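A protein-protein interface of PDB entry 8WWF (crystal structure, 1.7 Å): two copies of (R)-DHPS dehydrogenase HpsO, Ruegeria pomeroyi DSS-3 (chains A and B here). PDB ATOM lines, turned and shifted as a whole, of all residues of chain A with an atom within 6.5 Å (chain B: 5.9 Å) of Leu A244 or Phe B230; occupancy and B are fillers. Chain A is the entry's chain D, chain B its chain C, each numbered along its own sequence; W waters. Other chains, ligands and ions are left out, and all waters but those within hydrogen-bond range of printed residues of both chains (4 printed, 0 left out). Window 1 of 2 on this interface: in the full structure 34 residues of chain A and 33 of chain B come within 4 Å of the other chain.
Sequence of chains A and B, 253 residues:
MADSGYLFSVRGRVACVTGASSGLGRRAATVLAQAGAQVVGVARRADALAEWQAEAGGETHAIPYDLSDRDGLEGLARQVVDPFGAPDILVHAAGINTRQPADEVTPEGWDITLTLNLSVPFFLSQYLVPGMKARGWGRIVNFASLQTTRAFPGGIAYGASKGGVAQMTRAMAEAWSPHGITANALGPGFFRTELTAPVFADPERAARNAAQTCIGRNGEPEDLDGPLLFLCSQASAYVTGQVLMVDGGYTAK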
ATOM      1  N   PHE A   8      11.821 -20.634   7.016  1.00  0.00           N
ATOM      2  CA  PHE A   8      12.697 -21.170   8.141  1.00  0.00           C
ATOM      3  C   PHE A   8      14.189 -21.218   7.737  1.00  0.00           C
ATOM      4  O   PHE A   8      15.020 -21.821   8.413  1.00  0.00           O
ATOM      5  CB  PHE A   8      12.206 -22.563   8.533  1.00  0.00           C
ATOM      6  CG  PHE A   8      10.788 -22.567   9.021  1.00  0.00           C
ATOM      7  CD1 PHE A   8       9.731 -22.826   8.183  1.00  0.00           C
ATOM      8  CD2 PHE A   8      10.509 -22.310  10.348  1.00  0.00           C
ATOM      9  CE1 PHE A   8       8.437 -22.851   8.625  1.00  0.00           C
ATOM     10  CE2 PHE A   8       9.239 -22.289  10.793  1.00  0.00           C
ATOM     11  CZ  PHE A   8       8.184 -22.529   9.972  1.00  0.00           C
ATOM     12  N   ALA A 144      17.235 -20.041  28.161  1.00  0.00           N
ATOM     13  CA  ALA A 144      16.529 -20.080  29.496  1.00  0.00           C
ATOM     14  C   ALA A 144      16.589 -21.526  29.969  1.00  0.00           C
ATOM     15  O   ALA A 144      17.360 -22.309  29.456  1.00  0.00           O
ATOM     16  CB  ALA A 144      15.090 -19.598  29.305  1.00  0.00           C
ATOM     17  N   ASN A 184      14.771 -13.838  21.783  1.00  0.00           N
ATOM     18  CA  ASN A 184      13.956 -14.803  22.439  1.00  0.00           C
ATOM     19  C   ASN A 184      14.857 -15.747  23.137  1.00  0.00           C
ATOM     20  O   ASN A 184      16.081 -15.711  22.955  1.00  0.00           O
ATOM     21  CB  ASN A 184      13.080 -15.560  21.434  1.00  0.00           C
ATOM     22  CG  ASN A 184      12.088 -14.683  20.731  1.00  0.00           C
ATOM     23  OD1 ASN A 184      11.047 -14.247  21.326  1.00  0.00           O
ATOM     24  ND2 ASN A 184      12.408 -14.339  19.516  1.00  0.00           N
ATOM     25  N   ALA A 185      14.285 -16.581  23.978  1.00  0.00           N
ATOM     26  CA  ALA A 185      15.059 -17.548  24.735  1.00  0.00           C
ATOM     27  C   ALA A 185      14.499 -18.935  24.498  1.00  0.00           C
ATOM     28  O   ALA A 185      13.341 -19.147  24.671  1.00  0.00           O
ATOM     29  CB  ALA A 185      15.039 -17.250  26.207  1.00  0.00           C
ATOM     30  N   LEU A 186      15.340 -19.895  24.139  1.00  0.00           N
ATOM     31  CA  LEU A 186      14.928 -21.278  24.135  1.00  0.00           C
ATOM     32  C   LEU A 186      15.126 -21.765  25.516  1.00  0.00           C
ATOM     33  O   LEU A 186      16.207 -21.557  26.083  1.00  0.00           O
ATOM     34  CB  LEU A 186      15.832 -22.128  23.223  1.00  0.00           C
ATOM     35  CG  LEU A 186      15.659 -22.131  21.739  1.00  0.00           C
ATOM     36  CD1 LEU A 186      16.873 -22.846  21.103  1.00  0.00           C
ATOM     37  CD2 LEU A 186      14.264 -22.572  21.336  1.00  0.00           C
ATOM     38  N   GLY A 187      14.149 -22.514  26.003  1.00  0.00           N
ATOM     39  CA  GLY A 187      14.151 -23.179  27.258  1.00  0.00           C
ATOM     40  C   GLY A 187      14.146 -24.659  27.202  1.00  0.00           C
ATOM     41  O   GLY A 187      13.110 -25.298  27.301  1.00  0.00           O
ATOM     42  N   PRO A 188      15.333 -25.241  27.054  1.00  0.00           N
ATOM     43  CA  PRO A 188      15.390 -26.684  27.034  1.00  0.00           C
ATOM     44  C   PRO A 188      15.018 -27.276  28.377  1.00  0.00           C
ATOM     45  O   PRO A 188      15.265 -26.656  29.425  1.00  0.00           O
ATOM     46  CB  PRO A 188      16.865 -26.987  26.755  1.00  0.00           C
ATOM     47  CG  PRO A 188      17.590 -25.685  26.919  1.00  0.00           C
ATOM     48  CD  PRO A 188      16.639 -24.599  27.027  1.00  0.00           C
ATOM     49  N   GLY A 226      14.373 -27.824  15.325  1.00  0.00           N
ATOM     50  CA  GLY A 226      13.224 -27.110  14.862  1.00  0.00           C
ATOM     51  C   GLY A 226      13.034 -25.792  15.591  1.00  0.00           C
ATOM     52  O   GLY A 226      12.925 -24.717  14.969  1.00  0.00           O
ATOM     53  N   PRO A 227      12.942 -25.881  16.918  1.00  0.00           N
ATOM     54  CA  PRO A 227      12.817 -24.625  17.669  1.00  0.00           C
ATOM     55  C   PRO A 227      13.932 -23.605  17.426  1.00  0.00           C
ATOM     56  O   PRO A 227      13.616 -22.430  17.297  1.00  0.00           O
ATOM     57  CB  PRO A 227      12.888 -25.116  19.097  1.00  0.00           C
ATOM     58  CG  PRO A 227      12.210 -26.485  19.002  1.00  0.00           C
ATOM     59  CD  PRO A 227      12.809 -27.056  17.772  1.00  0.00           C
ATOM     60  N   LEU A 228      15.160 -24.044  17.265  1.00  0.00           N
ATOM     61  CA  LEU A 228      16.272 -23.171  16.990  1.00  0.00           C
ATOM     62  C   LEU A 228      16.110 -22.492  15.662  1.00  0.00           C
ATOM     63  O   LEU A 228      16.191 -21.260  15.551  1.00  0.00           O
ATOM     64  CB  LEU A 228      17.594 -23.935  17.045  1.00  0.00           C
ATOM     65  CG  LEU A 228      18.812 -23.080  16.658  1.00  0.00           C
ATOM     66  CD1 LEU A 228      19.164 -22.059  17.734  1.00  0.00           C
ATOM     67  CD2 LEU A 228      19.960 -24.045  16.391  1.00  0.00           C
ATOM     68  N   PHE A 230      13.491 -22.107  13.833  1.00  0.00           N
ATOM     69  CA  PHE A 230      12.330 -21.159  13.927  1.00  0.00           C
ATOM     70  C   PHE A 230      12.724 -19.777  14.487  1.00  0.00           C
ATOM     71  O   PHE A 230      12.392 -18.748  13.924  1.00  0.00           O
ATOM     72  CB  PHE A 230      11.249 -21.824  14.818  1.00  0.00           C
ATOM     73  CG  PHE A 230      10.125 -20.914  15.181  1.00  0.00           C
ATOM     74  CD1 PHE A 230       9.354 -20.323  14.218  1.00  0.00           C
ATOM     75  CD2 PHE A 230       9.783 -20.690  16.511  1.00  0.00           C
ATOM     76  CE1 PHE A 230       8.277 -19.492  14.499  1.00  0.00           C
ATOM     77  CE2 PHE A 230       8.706 -19.886  16.808  1.00  0.00           C
ATOM     78  CZ  PHE A 230       7.983 -19.253  15.823  1.00  0.00           C
ATOM     79  N   LEU A 231      13.417 -19.769  15.612  1.00  0.00           N
ATOM     80  CA  LEU A 231      13.926 -18.562  16.296  1.00  0.00           C
ATOM     81  C   LEU A 231      15.066 -17.851  15.625  1.00  0.00           C
ATOM     82  O   LEU A 231      15.364 -16.717  15.977  1.00  0.00           O
ATOM     83  CB  LEU A 231      14.311 -18.821  17.741  1.00  0.00           C
ATOM     84  CG  LEU A 231      13.159 -19.246  18.669  1.00  0.00           C
ATOM     85  CD1 LEU A 231      13.626 -19.408  20.062  1.00  0.00           C
ATOM     86  CD2 LEU A 231      12.014 -18.280  18.637  1.00  0.00           C
ATOM     87  N   ALA A 235      10.552 -16.860   9.820  1.00  0.00           N
ATOM     88  CA  ALA A 235       9.365 -17.480  10.387  1.00  0.00           C
ATOM     89  C   ALA A 235       8.936 -16.823  11.708  1.00  0.00           C
ATOM     90  O   ALA A 235       7.768 -16.782  11.950  1.00  0.00           O
ATOM     91  CB  ALA A 235       9.533 -18.978  10.609  1.00  0.00           C
ATOM     92  N   GLN A 242      10.115 -13.523  23.952  1.00  0.00           N
ATOM     93  CA  GLN A 242       9.438 -14.732  24.435  1.00  0.00           C
ATOM     94  C   GLN A 242      10.466 -15.794  24.921  1.00  0.00           C
ATOM     95  O   GLN A 242      11.607 -15.817  24.483  1.00  0.00           O
ATOM     96  CB  GLN A 242       8.612 -15.388  23.334  1.00  0.00           C
ATOM     97  CG  GLN A 242       7.544 -14.428  22.770  1.00  0.00           C
ATOM     98  CD  GLN A 242       6.674 -13.769  23.840  1.00  0.00           C
ATOM     99  OE1 GLN A 242       6.002 -14.460  24.670  1.00  0.00           O
ATOM    100  NE2 GLN A 242       6.632 -12.413  23.824  1.00  0.00           N
ATOM    101  N   VAL A 243       9.992 -16.642  25.859  1.00  0.00           N
ATOM    102  CA  VAL A 243      10.701 -17.872  26.279  1.00  0.00           C
ATOM    103  C   VAL A 243       9.913 -19.041  25.660  1.00  0.00           C
ATOM    104  O   VAL A 243       8.701 -19.148  25.848  1.00  0.00           O
ATOM    105  CB  VAL A 243      10.725 -18.020  27.746  1.00  0.00           C
ATOM    106  CG1 VAL A 243      11.300 -19.360  28.104  1.00  0.00           C
ATOM    107  CG2 VAL A 243      11.374 -16.836  28.436  1.00  0.00           C
ATOM    108  N   LEU A 244      10.572 -19.809  24.831  1.00  0.00           N
ATOM    109  CA  LEU A 244       9.990 -20.986  24.161  1.00  0.00           C
ATOM    110  C   LEU A 244      10.529 -22.244  24.817  1.00  0.00           C
ATOM    111  O   LEU A 244      11.700 -22.559  24.636  1.00  0.00           O
ATOM    112  CB  LEU A 244      10.360 -20.985  22.673  1.00  0.00           C
ATOM    113  CG  LEU A 244       9.930 -22.127  21.803  1.00  0.00           C
ATOM    114  CD1 LEU A 244       8.472 -22.388  22.010  1.00  0.00           C
ATOM    115  CD2 LEU A 244      10.186 -21.874  20.313  1.00  0.00           C
ATOM    116  N   MET A 245       9.715 -22.896  25.669  1.00  0.00           N
ATOM    117  CA  MET A 245      10.152 -24.080  26.369  1.00  0.00           C
ATOM    118  C   MET A 245      10.139 -25.308  25.435  1.00  0.00           C
ATOM    119  O   MET A 245       9.127 -25.542  24.725  1.00  0.00           O
ATOM    120  CB  MET A 245       9.270 -24.373  27.595  1.00  0.00           C
ATOM    121  CG  MET A 245       9.281 -23.312  28.680  1.00  0.00           C
ATOM    122  SD  MET A 245      10.881 -22.825  29.230  1.00  0.00           S
ATOM    123  CE  MET A 245      11.412 -24.331  30.060  1.00  0.00           C
ATOM    124  N   VAL A 246      11.229 -26.067  25.426  1.00  0.00           N
ATOM    125  CA  VAL A 246      11.374 -27.281  24.572  1.00  0.00           C
ATOM    126  C   VAL A 246      11.708 -28.325  25.621  1.00  0.00           C
ATOM    127  O   VAL A 246      12.880 -28.675  25.857  1.00  0.00           O
ATOM    128  CB  VAL A 246      12.479 -27.153  23.519  1.00  0.00           C
ATOM    129  CG1 VAL A 246      12.494 -28.333  22.598  1.00  0.00           C
ATOM    130  CG2 VAL A 246      12.296 -25.793  22.751  1.00  0.00           C
ATOM    131  N   PHE B   8       9.748 -28.834   8.893  1.00  0.00           N
ATOM    132  CA  PHE B   8       8.605 -27.912   9.054  1.00  0.00           C
ATOM    133  C   PHE B   8       7.453 -28.233   8.073  1.00  0.00           C
ATOM    134  O   PHE B   8       6.468 -27.456   7.946  1.00  0.00           O
ATOM    135  CB  PHE B   8       9.059 -26.457   8.820  1.00  0.00           C
ATOM    136  CG  PHE B   8      10.089 -26.001   9.823  1.00  0.00           C
ATOM    137  CD1 PHE B   8      11.422 -25.993   9.514  1.00  0.00           C
ATOM    138  CD2 PHE B   8       9.709 -25.591  11.097  1.00  0.00           C
ATOM    139  CE1 PHE B   8      12.378 -25.650  10.414  1.00  0.00           C
ATOM    140  CE2 PHE B   8      10.673 -25.210  11.989  1.00  0.00           C
ATOM    141  CZ  PHE B   8      11.992 -25.242  11.669  1.00  0.00           C
ATOM    142  N   ARG B 139      -1.153 -33.071  16.129  1.00  0.00           N
ATOM    143  CA  ARG B 139      -0.861 -31.708  16.517  1.00  0.00           C
ATOM    144  C   ARG B 139      -2.207 -31.004  16.713  1.00  0.00           C
ATOM    145  O   ARG B 139      -3.057 -30.858  15.800  1.00  0.00           O
ATOM    146  CB  ARG B 139      -0.076 -31.051  15.372  1.00  0.00           C
ATOM    147  CG  ARG B 139       1.272 -31.607  15.132  1.00  0.00           C
ATOM    148  CD  ARG B 139       2.302 -31.212  16.205  1.00  0.00           C
ATOM    149  NE  ARG B 139       3.652 -31.638  15.901  1.00  0.00           N
ATOM    150  CZ  ARG B 139       4.168 -32.839  16.194  1.00  0.00           C
ATOM    151  NH1 ARG B 139       3.414 -33.801  16.786  1.00  0.00           N
ATOM    152  NH2 ARG B 139       5.434 -33.084  15.991  1.00  0.00           N
ATOM    153  N   ASP B 225       2.056 -17.313   9.768  1.00  0.00           N
ATOM    154  CA  ASP B 225       2.400 -18.491   9.021  1.00  0.00           C
ATOM    155  C   ASP B 225       3.473 -19.369   9.619  1.00  0.00           C
ATOM    156  O   ASP B 225       3.294 -20.594   9.735  1.00  0.00           O
ATOM    157  CB  ASP B 225       2.823 -18.111   7.601  1.00  0.00           C
ATOM    158  CG  ASP B 225       1.790 -17.208   6.857  1.00  0.00           C
ATOM    159  OD1 ASP B 225       0.700 -16.885   7.350  1.00  0.00           O
ATOM    160  OD2 ASP B 225       2.096 -16.855   5.651  1.00  0.00           O
ATOM    161  N   GLY B 226       4.600 -18.783   9.983  1.00  0.00           N
ATOM    162  CA  GLY B 226       5.774 -19.494  10.492  1.00  0.00           C
ATOM    163  C   GLY B 226       5.435 -20.151  11.814  1.00  0.00           C
ATOM    164  O   GLY B 226       5.696 -21.344  12.020  1.00  0.00           O
ATOM    165  N   PRO B 227       4.890 -19.351  12.747  1.00  0.00           N
ATOM    166  CA  PRO B 227       4.584 -19.987  14.038  1.00  0.00           C
ATOM    167  C   PRO B 227       3.555 -21.129  13.949  1.00  0.00           C
ATOM    168  O   PRO B 227       3.699 -22.165  14.610  1.00  0.00           O
ATOM    169  CB  PRO B 227       3.998 -18.836  14.836  1.00  0.00           C
ATOM    170  CG  PRO B 227       4.756 -17.618  14.298  1.00  0.00           C
ATOM    171  CD  PRO B 227       4.848 -17.881  12.812  1.00  0.00           C
ATOM    172  N   LEU B 228       2.574 -20.954  13.108  1.00  0.00           N
ATOM    173  CA  LEU B 228       1.631 -22.047  12.773  1.00  0.00           C
ATOM    174  C   LEU B 228       2.278 -23.292  12.231  1.00  0.00           C
ATOM    175  O   LEU B 228       2.090 -24.411  12.785  1.00  0.00           O
ATOM    176  CB  LEU B 228       0.534 -21.609  11.850  1.00  0.00           C
ATOM    177  CG  LEU B 228      -0.471 -22.686  11.475  1.00  0.00           C
ATOM    178  CD1 LEU B 228      -1.438 -22.994  12.583  1.00  0.00           C
ATOM    179  CD2 LEU B 228      -1.208 -22.155  10.276  1.00  0.00           C
ATOM    180  N   LEU B 229       3.089 -23.142  11.189  1.00  0.00           N
ATOM    181  CA  LEU B 229       3.695 -24.321  10.621  1.00  0.00           C
ATOM    182  C   LEU B 229       4.645 -25.014  11.577  1.00  0.00           C
ATOM    183  O   LEU B 229       4.704 -26.212  11.637  1.00  0.00           O
ATOM    184  CB  LEU B 229       4.407 -23.927   9.298  1.00  0.00           C
ATOM    185  CG  LEU B 229       3.468 -23.542   8.145  1.00  0.00           C
ATOM    186  CD1 LEU B 229       4.261 -22.837   7.068  1.00  0.00           C
ATOM    187  CD2 LEU B 229       2.812 -24.800   7.607  1.00  0.00           C
ATOM    188  N   PHE B 230       5.336 -24.236  12.408  1.00  0.00           N
ATOM    189  CA  PHE B 230       6.207 -24.781  13.432  1.00  0.00           C
ATOM    190  C   PHE B 230       5.388 -25.685  14.353  1.00  0.00           C
ATOM    191  O   PHE B 230       5.802 -26.824  14.639  1.00  0.00           O
ATOM    192  CB  PHE B 230       6.821 -23.566  14.241  1.00  0.00           C
ATOM    193  CG  PHE B 230       7.500 -23.988  15.493  1.00  0.00           C
ATOM    194  CD1 PHE B 230       8.545 -24.888  15.452  1.00  0.00           C
ATOM    195  CD2 PHE B 230       7.106 -23.513  16.756  1.00  0.00           C
ATOM    196  CE1 PHE B 230       9.172 -25.317  16.582  1.00  0.00           C
ATOM    197  CE2 PHE B 230       7.779 -23.915  17.875  1.00  0.00           C
ATOM    198  CZ  PHE B 230       8.796 -24.828  17.814  1.00  0.00           C
ATOM    199  N   LEU B 231       4.233 -25.190  14.836  1.00  0.00           N
ATOM    200  CA  LEU B 231       3.359 -25.949  15.759  1.00  0.00           C
ATOM    201  C   LEU B 231       2.599 -27.125  15.157  1.00  0.00           C
ATOM    202  O   LEU B 231       1.905 -27.865  15.835  1.00  0.00           O
ATOM    203  CB  LEU B 231       2.405 -25.026  16.516  1.00  0.00           C
ATOM    204  CG  LEU B 231       3.093 -24.013  17.500  1.00  0.00           C
ATOM    205  CD1 LEU B 231       1.978 -23.263  18.125  1.00  0.00           C
ATOM    206  CD2 LEU B 231       3.922 -24.725  18.541  1.00  0.00           C
ATOM    207  N   CYS B 232       2.625 -27.211  13.841  1.00  0.00           N
ATOM    208  CA  CYS B 232       1.881 -28.224  13.078  1.00  0.00           C
ATOM    209  C   CYS B 232       2.810 -29.230  12.426  1.00  0.00           C
ATOM    210  O   CYS B 232       2.301 -30.188  11.711  1.00  0.00           O
ATOM    211  CB  CYS B 232       1.081 -27.546  11.966  1.00  0.00           C
ATOM    212  SG  CYS B 232      -0.332 -26.646  12.525  1.00  0.00           S
ATOM    213  N   SER B 233       4.067 -29.236  12.778  1.00  0.00           N
ATOM    214  CA  SER B 233       5.085 -30.086  12.156  1.00  0.00           C
ATOM    215  C   SER B 233       6.004 -30.854  13.041  1.00  0.00           C
ATOM    216  O   SER B 233       5.992 -30.657  14.273  1.00  0.00           O
ATOM    217  CB  SER B 233       5.875 -29.221  11.161  1.00  0.00           C
ATOM    218  OG  SER B 233       6.676 -28.253  11.788  1.00  0.00           O
ATOM    219  N   GLN B 234       6.891 -31.629  12.441  1.00  0.00           N
ATOM    220  CA  GLN B 234       7.861 -32.407  13.181  1.00  0.00           C
ATOM    221  C   GLN B 234       8.792 -31.542  14.017  1.00  0.00           C
ATOM    222  O   GLN B 234       9.277 -31.991  15.068  1.00  0.00           O
ATOM    223  CB  GLN B 234       8.663 -33.358  12.313  1.00  0.00           C
ATOM    224  CG  GLN B 234       9.420 -34.389  13.136  1.00  0.00           C
ATOM    225  CD  GLN B 234       8.655 -35.315  14.190  1.00  0.00           C
ATOM    226  OE1 GLN B 234       7.396 -35.390  14.375  1.00  0.00           O
ATOM    227  NE2 GLN B 234       9.498 -36.010  14.967  1.00  0.00           N
ATOM    228  N   ALA B 235       9.000 -30.308  13.579  1.00  0.00           N
ATOM    229  CA  ALA B 235       9.903 -29.377  14.223  1.00  0.00           C
ATOM    230  C   ALA B 235       9.569 -29.191  15.670  1.00  0.00           C
ATOM    231  O   ALA B 235      10.447 -28.871  16.441  1.00  0.00           O
ATOM    232  CB  ALA B 235       9.854 -28.031  13.530  1.00  0.00           C
ATOM    233  N   SER B 236       8.295 -29.280  16.016  1.00  0.00           N
ATOM    234  CA  SER B 236       7.855 -29.035  17.421  1.00  0.00           C
ATOM    235  C   SER B 236       7.521 -30.280  18.208  1.00  0.00           C
ATOM    236  O   SER B 236       6.793 -30.230  19.177  1.00  0.00           O
ATOM    237  CB  SER B 236       6.623 -28.121  17.373  1.00  0.00           C
ATOM    238  OG  SER B 236       5.487 -28.625  16.651  1.00  0.00           O
ATOM    239  N   VAL B 239       7.852 -29.924  21.934  1.00  0.00           N
ATOM    240  CA  VAL B 239       7.171 -28.692  22.426  1.00  0.00           C
ATOM    241  C   VAL B 239       5.714 -29.076  22.616  1.00  0.00           C
ATOM    242  O   VAL B 239       4.977 -29.415  21.664  1.00  0.00           O
ATOM    243  CB  VAL B 239       7.295 -27.511  21.466  1.00  0.00           C
ATOM    244  CG1 VAL B 239       6.468 -26.315  21.987  1.00  0.00           C
ATOM    245  CG2 VAL B 239       8.748 -27.068  21.220  1.00  0.00           C
ATOM    246  N   GLN B 242       2.429 -25.607  25.647  1.00  0.00           N
ATOM    247  CA  GLN B 242       2.985 -24.278  25.608  1.00  0.00           C
ATOM    248  C   GLN B 242       2.005 -23.272  24.967  1.00  0.00           C
ATOM    249  O   GLN B 242       1.243 -23.651  24.115  1.00  0.00           O
ATOM    250  CB  GLN B 242       4.331 -24.219  24.892  1.00  0.00           C
ATOM    251  CG  GLN B 242       5.351 -25.173  25.470  1.00  0.00           C
ATOM    252  CD  GLN B 242       5.555 -25.038  26.987  1.00  0.00           C
ATOM    253  OE1 GLN B 242       5.845 -23.941  27.550  1.00  0.00           O
ATOM    254  NE2 GLN B 242       5.421 -26.196  27.667  1.00  0.00           N
ATOM    255  N   LEU B 244       2.555 -19.949  22.764  1.00  0.00           N
ATOM    256  CA  LEU B 244       3.522 -19.261  21.980  1.00  0.00           C
ATOM    257  C   LEU B 244       2.927 -17.949  21.485  1.00  0.00           C
ATOM    258  O   LEU B 244       2.037 -17.958  20.640  1.00  0.00           O
ATOM    259  CB  LEU B 244       3.859 -20.100  20.710  1.00  0.00           C
ATOM    260  CG  LEU B 244       4.813 -19.457  19.710  1.00  0.00           C
ATOM    261  CD1 LEU B 244       6.043 -18.916  20.449  1.00  0.00           C
ATOM    262  CD2 LEU B 244       5.139 -20.477  18.584  1.00  0.00           C
HETATM  263  O   HOH W   1       7.626 -27.773  25.532  1.00  0.00           O
HETATM  264  O   HOH W   2       5.305 -16.026   9.631  1.00  0.00           O
HETATM  265  O   HOH W   3      13.529 -30.392  16.137  1.00  0.00           O
HETATM  266  O   HOH W   4       6.962 -21.988  26.114  1.00  0.00           O
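O of Ala A185 lies within hydrogen-bond range of N of Leu A244, at 2.9 Å. The backbone carbonyl oxygen of Phe B230 sits at hydrogen-bond distance from the side-chain hydroxyl of Ser B236 (2.7 Å). The backbone carbonyl oxygen (O) of Phe B230 is in hydrogen-bond range of the side-chain hydroxyl (OG) of Ser B233 (3.3 Å). N of Gly A187 is in hydrogen-bond range of O of Leu A244, at 2.8 Å.
Among the printed residues, pairs that only touch across the chains: Ala A235 with Pro B227 (3.2 Å), Pro A227 with Ala B235 (3.3 Å), Phe A8 with Phe B8 (3.3 Å), Phe A8 with Gly B226 (3.4 Å), Met A245 with Gln B242 (3.5 Å), Gly A226 with Phe B8 (3.5 Å), Gly A226 with Ala B235 (3.6 Å), Ala A235 with Gly B226 (3.7 Å), Phe A230 with Pro B227 (3.8 Å), Pro A227 with Phe B230 (3.8 Å), Met A245 with Val B239 (3.8 Å), Phe A230 with Phe B230 (3.9 Å), Phe A230 with Gly B226 (3.96 Å) and Leu A244 with Phe B230 (3.99 Å).
Of the printed residues of chain A, Phe B230 touches Pro A227 (3.8 Å), Phe A230 (3.9 Å) and Leu A244 (3.99 Å). Of the printed residues of chain B, Pro A227 touches Phe B230 and Ala B235. Printed residues of chain B within 4 Å of Ala A235: Gly B226 and Pro B227. Of the printed residues of chain A, Gly B226 touches Phe A8 (3.4 Å), Phe A230 (3.96 Å) and Ala A235 (3.7 Å). Of the printed residues of chain A, Val B239 touches Met A245. Of the printed residues of chain A, Pro B227 touches Phe A230 and Ala A235. Asn A184 touches none of the printed residues of chain B. The nearest printed residue of chain A that does not touch Phe B230 is Gly A226 (4.02 Å). The nearest printed residue of chain A that does not touch Ala B235 is Phe A8 (6.4 Å).
Of the 18 printed residues of chain A, 7 touch a printed residue of chain B. Hydrophobic or aromatic side chains of chain A that line the printed part of chain B: Phe A8, Pro A227, Phe A230, Ala A235, Leu A244 and Met A245. Of the 17 printed residues of chain B, 7 touch a printed residue of chain A. Printed residues of chain B that touch a printed residue of chain A: Phe B8, Gly B226, Pro B227, Phe B230, Ala B235, Val B239 and Gln B242. Hydrophobic or aromatic side chains of chain B that line the printed part of chain A: Phe B8, Pro B227, Phe B230, Ala B235 and Val B239. Along chain B the printed residues that touch a printed residue of chain A span positions 8 to 242. Among the printed residues, no Asp or Glu carboxylate lies within 4 Å of a Lys or Arg side-chain nitrogen of the other chain.
Phe A8 touches Gly B226, and with the chains exchanged Gly A226 touches Phe B8. Pro A227 touches Phe B230, and with the chains exchanged Phe A230 touches Pro B227. Phe A230 touches Gly B226, but with the chains exchanged Gly A226 does not touch Phe B230 (4.02 Å). Leu A244 touches Phe B230, but with the chains exchanged Phe A230 does not touch Leu B244 (4.03 Å). Positions printed for both chains: 8, 226, 227, 228, 230, 231, 235, 242 and 244. Of the 14 pairs that touch across the chains among the printed residues, 10 have their exchanged pair printed and touching as well.
Water W4 lies within hydrogen-bond range of the side-chain amide oxygen (OE1) of Gln B242 (2.7 Å), the backbone NH (N) of Met A245 (2.9 Å) and the backbone carbonyl oxygen (O) of Val A243 (3.3 Å). Water W1 lies within hydrogen-bond range of the backbone carbonyl oxygen of Met A245 and the side-chain amide nitrogen of Gln B242. Water W3 lies within hydrogen-bond range of the backbone NH (N) of Gly A226 (2.8 Å) and the backbone carbonyl oxygen (O) of Ala B235 (3.5 Å). Water W2 lies within hydrogen-bond range of N of Gly B226, O of Ala A235 and N of Asp B225.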
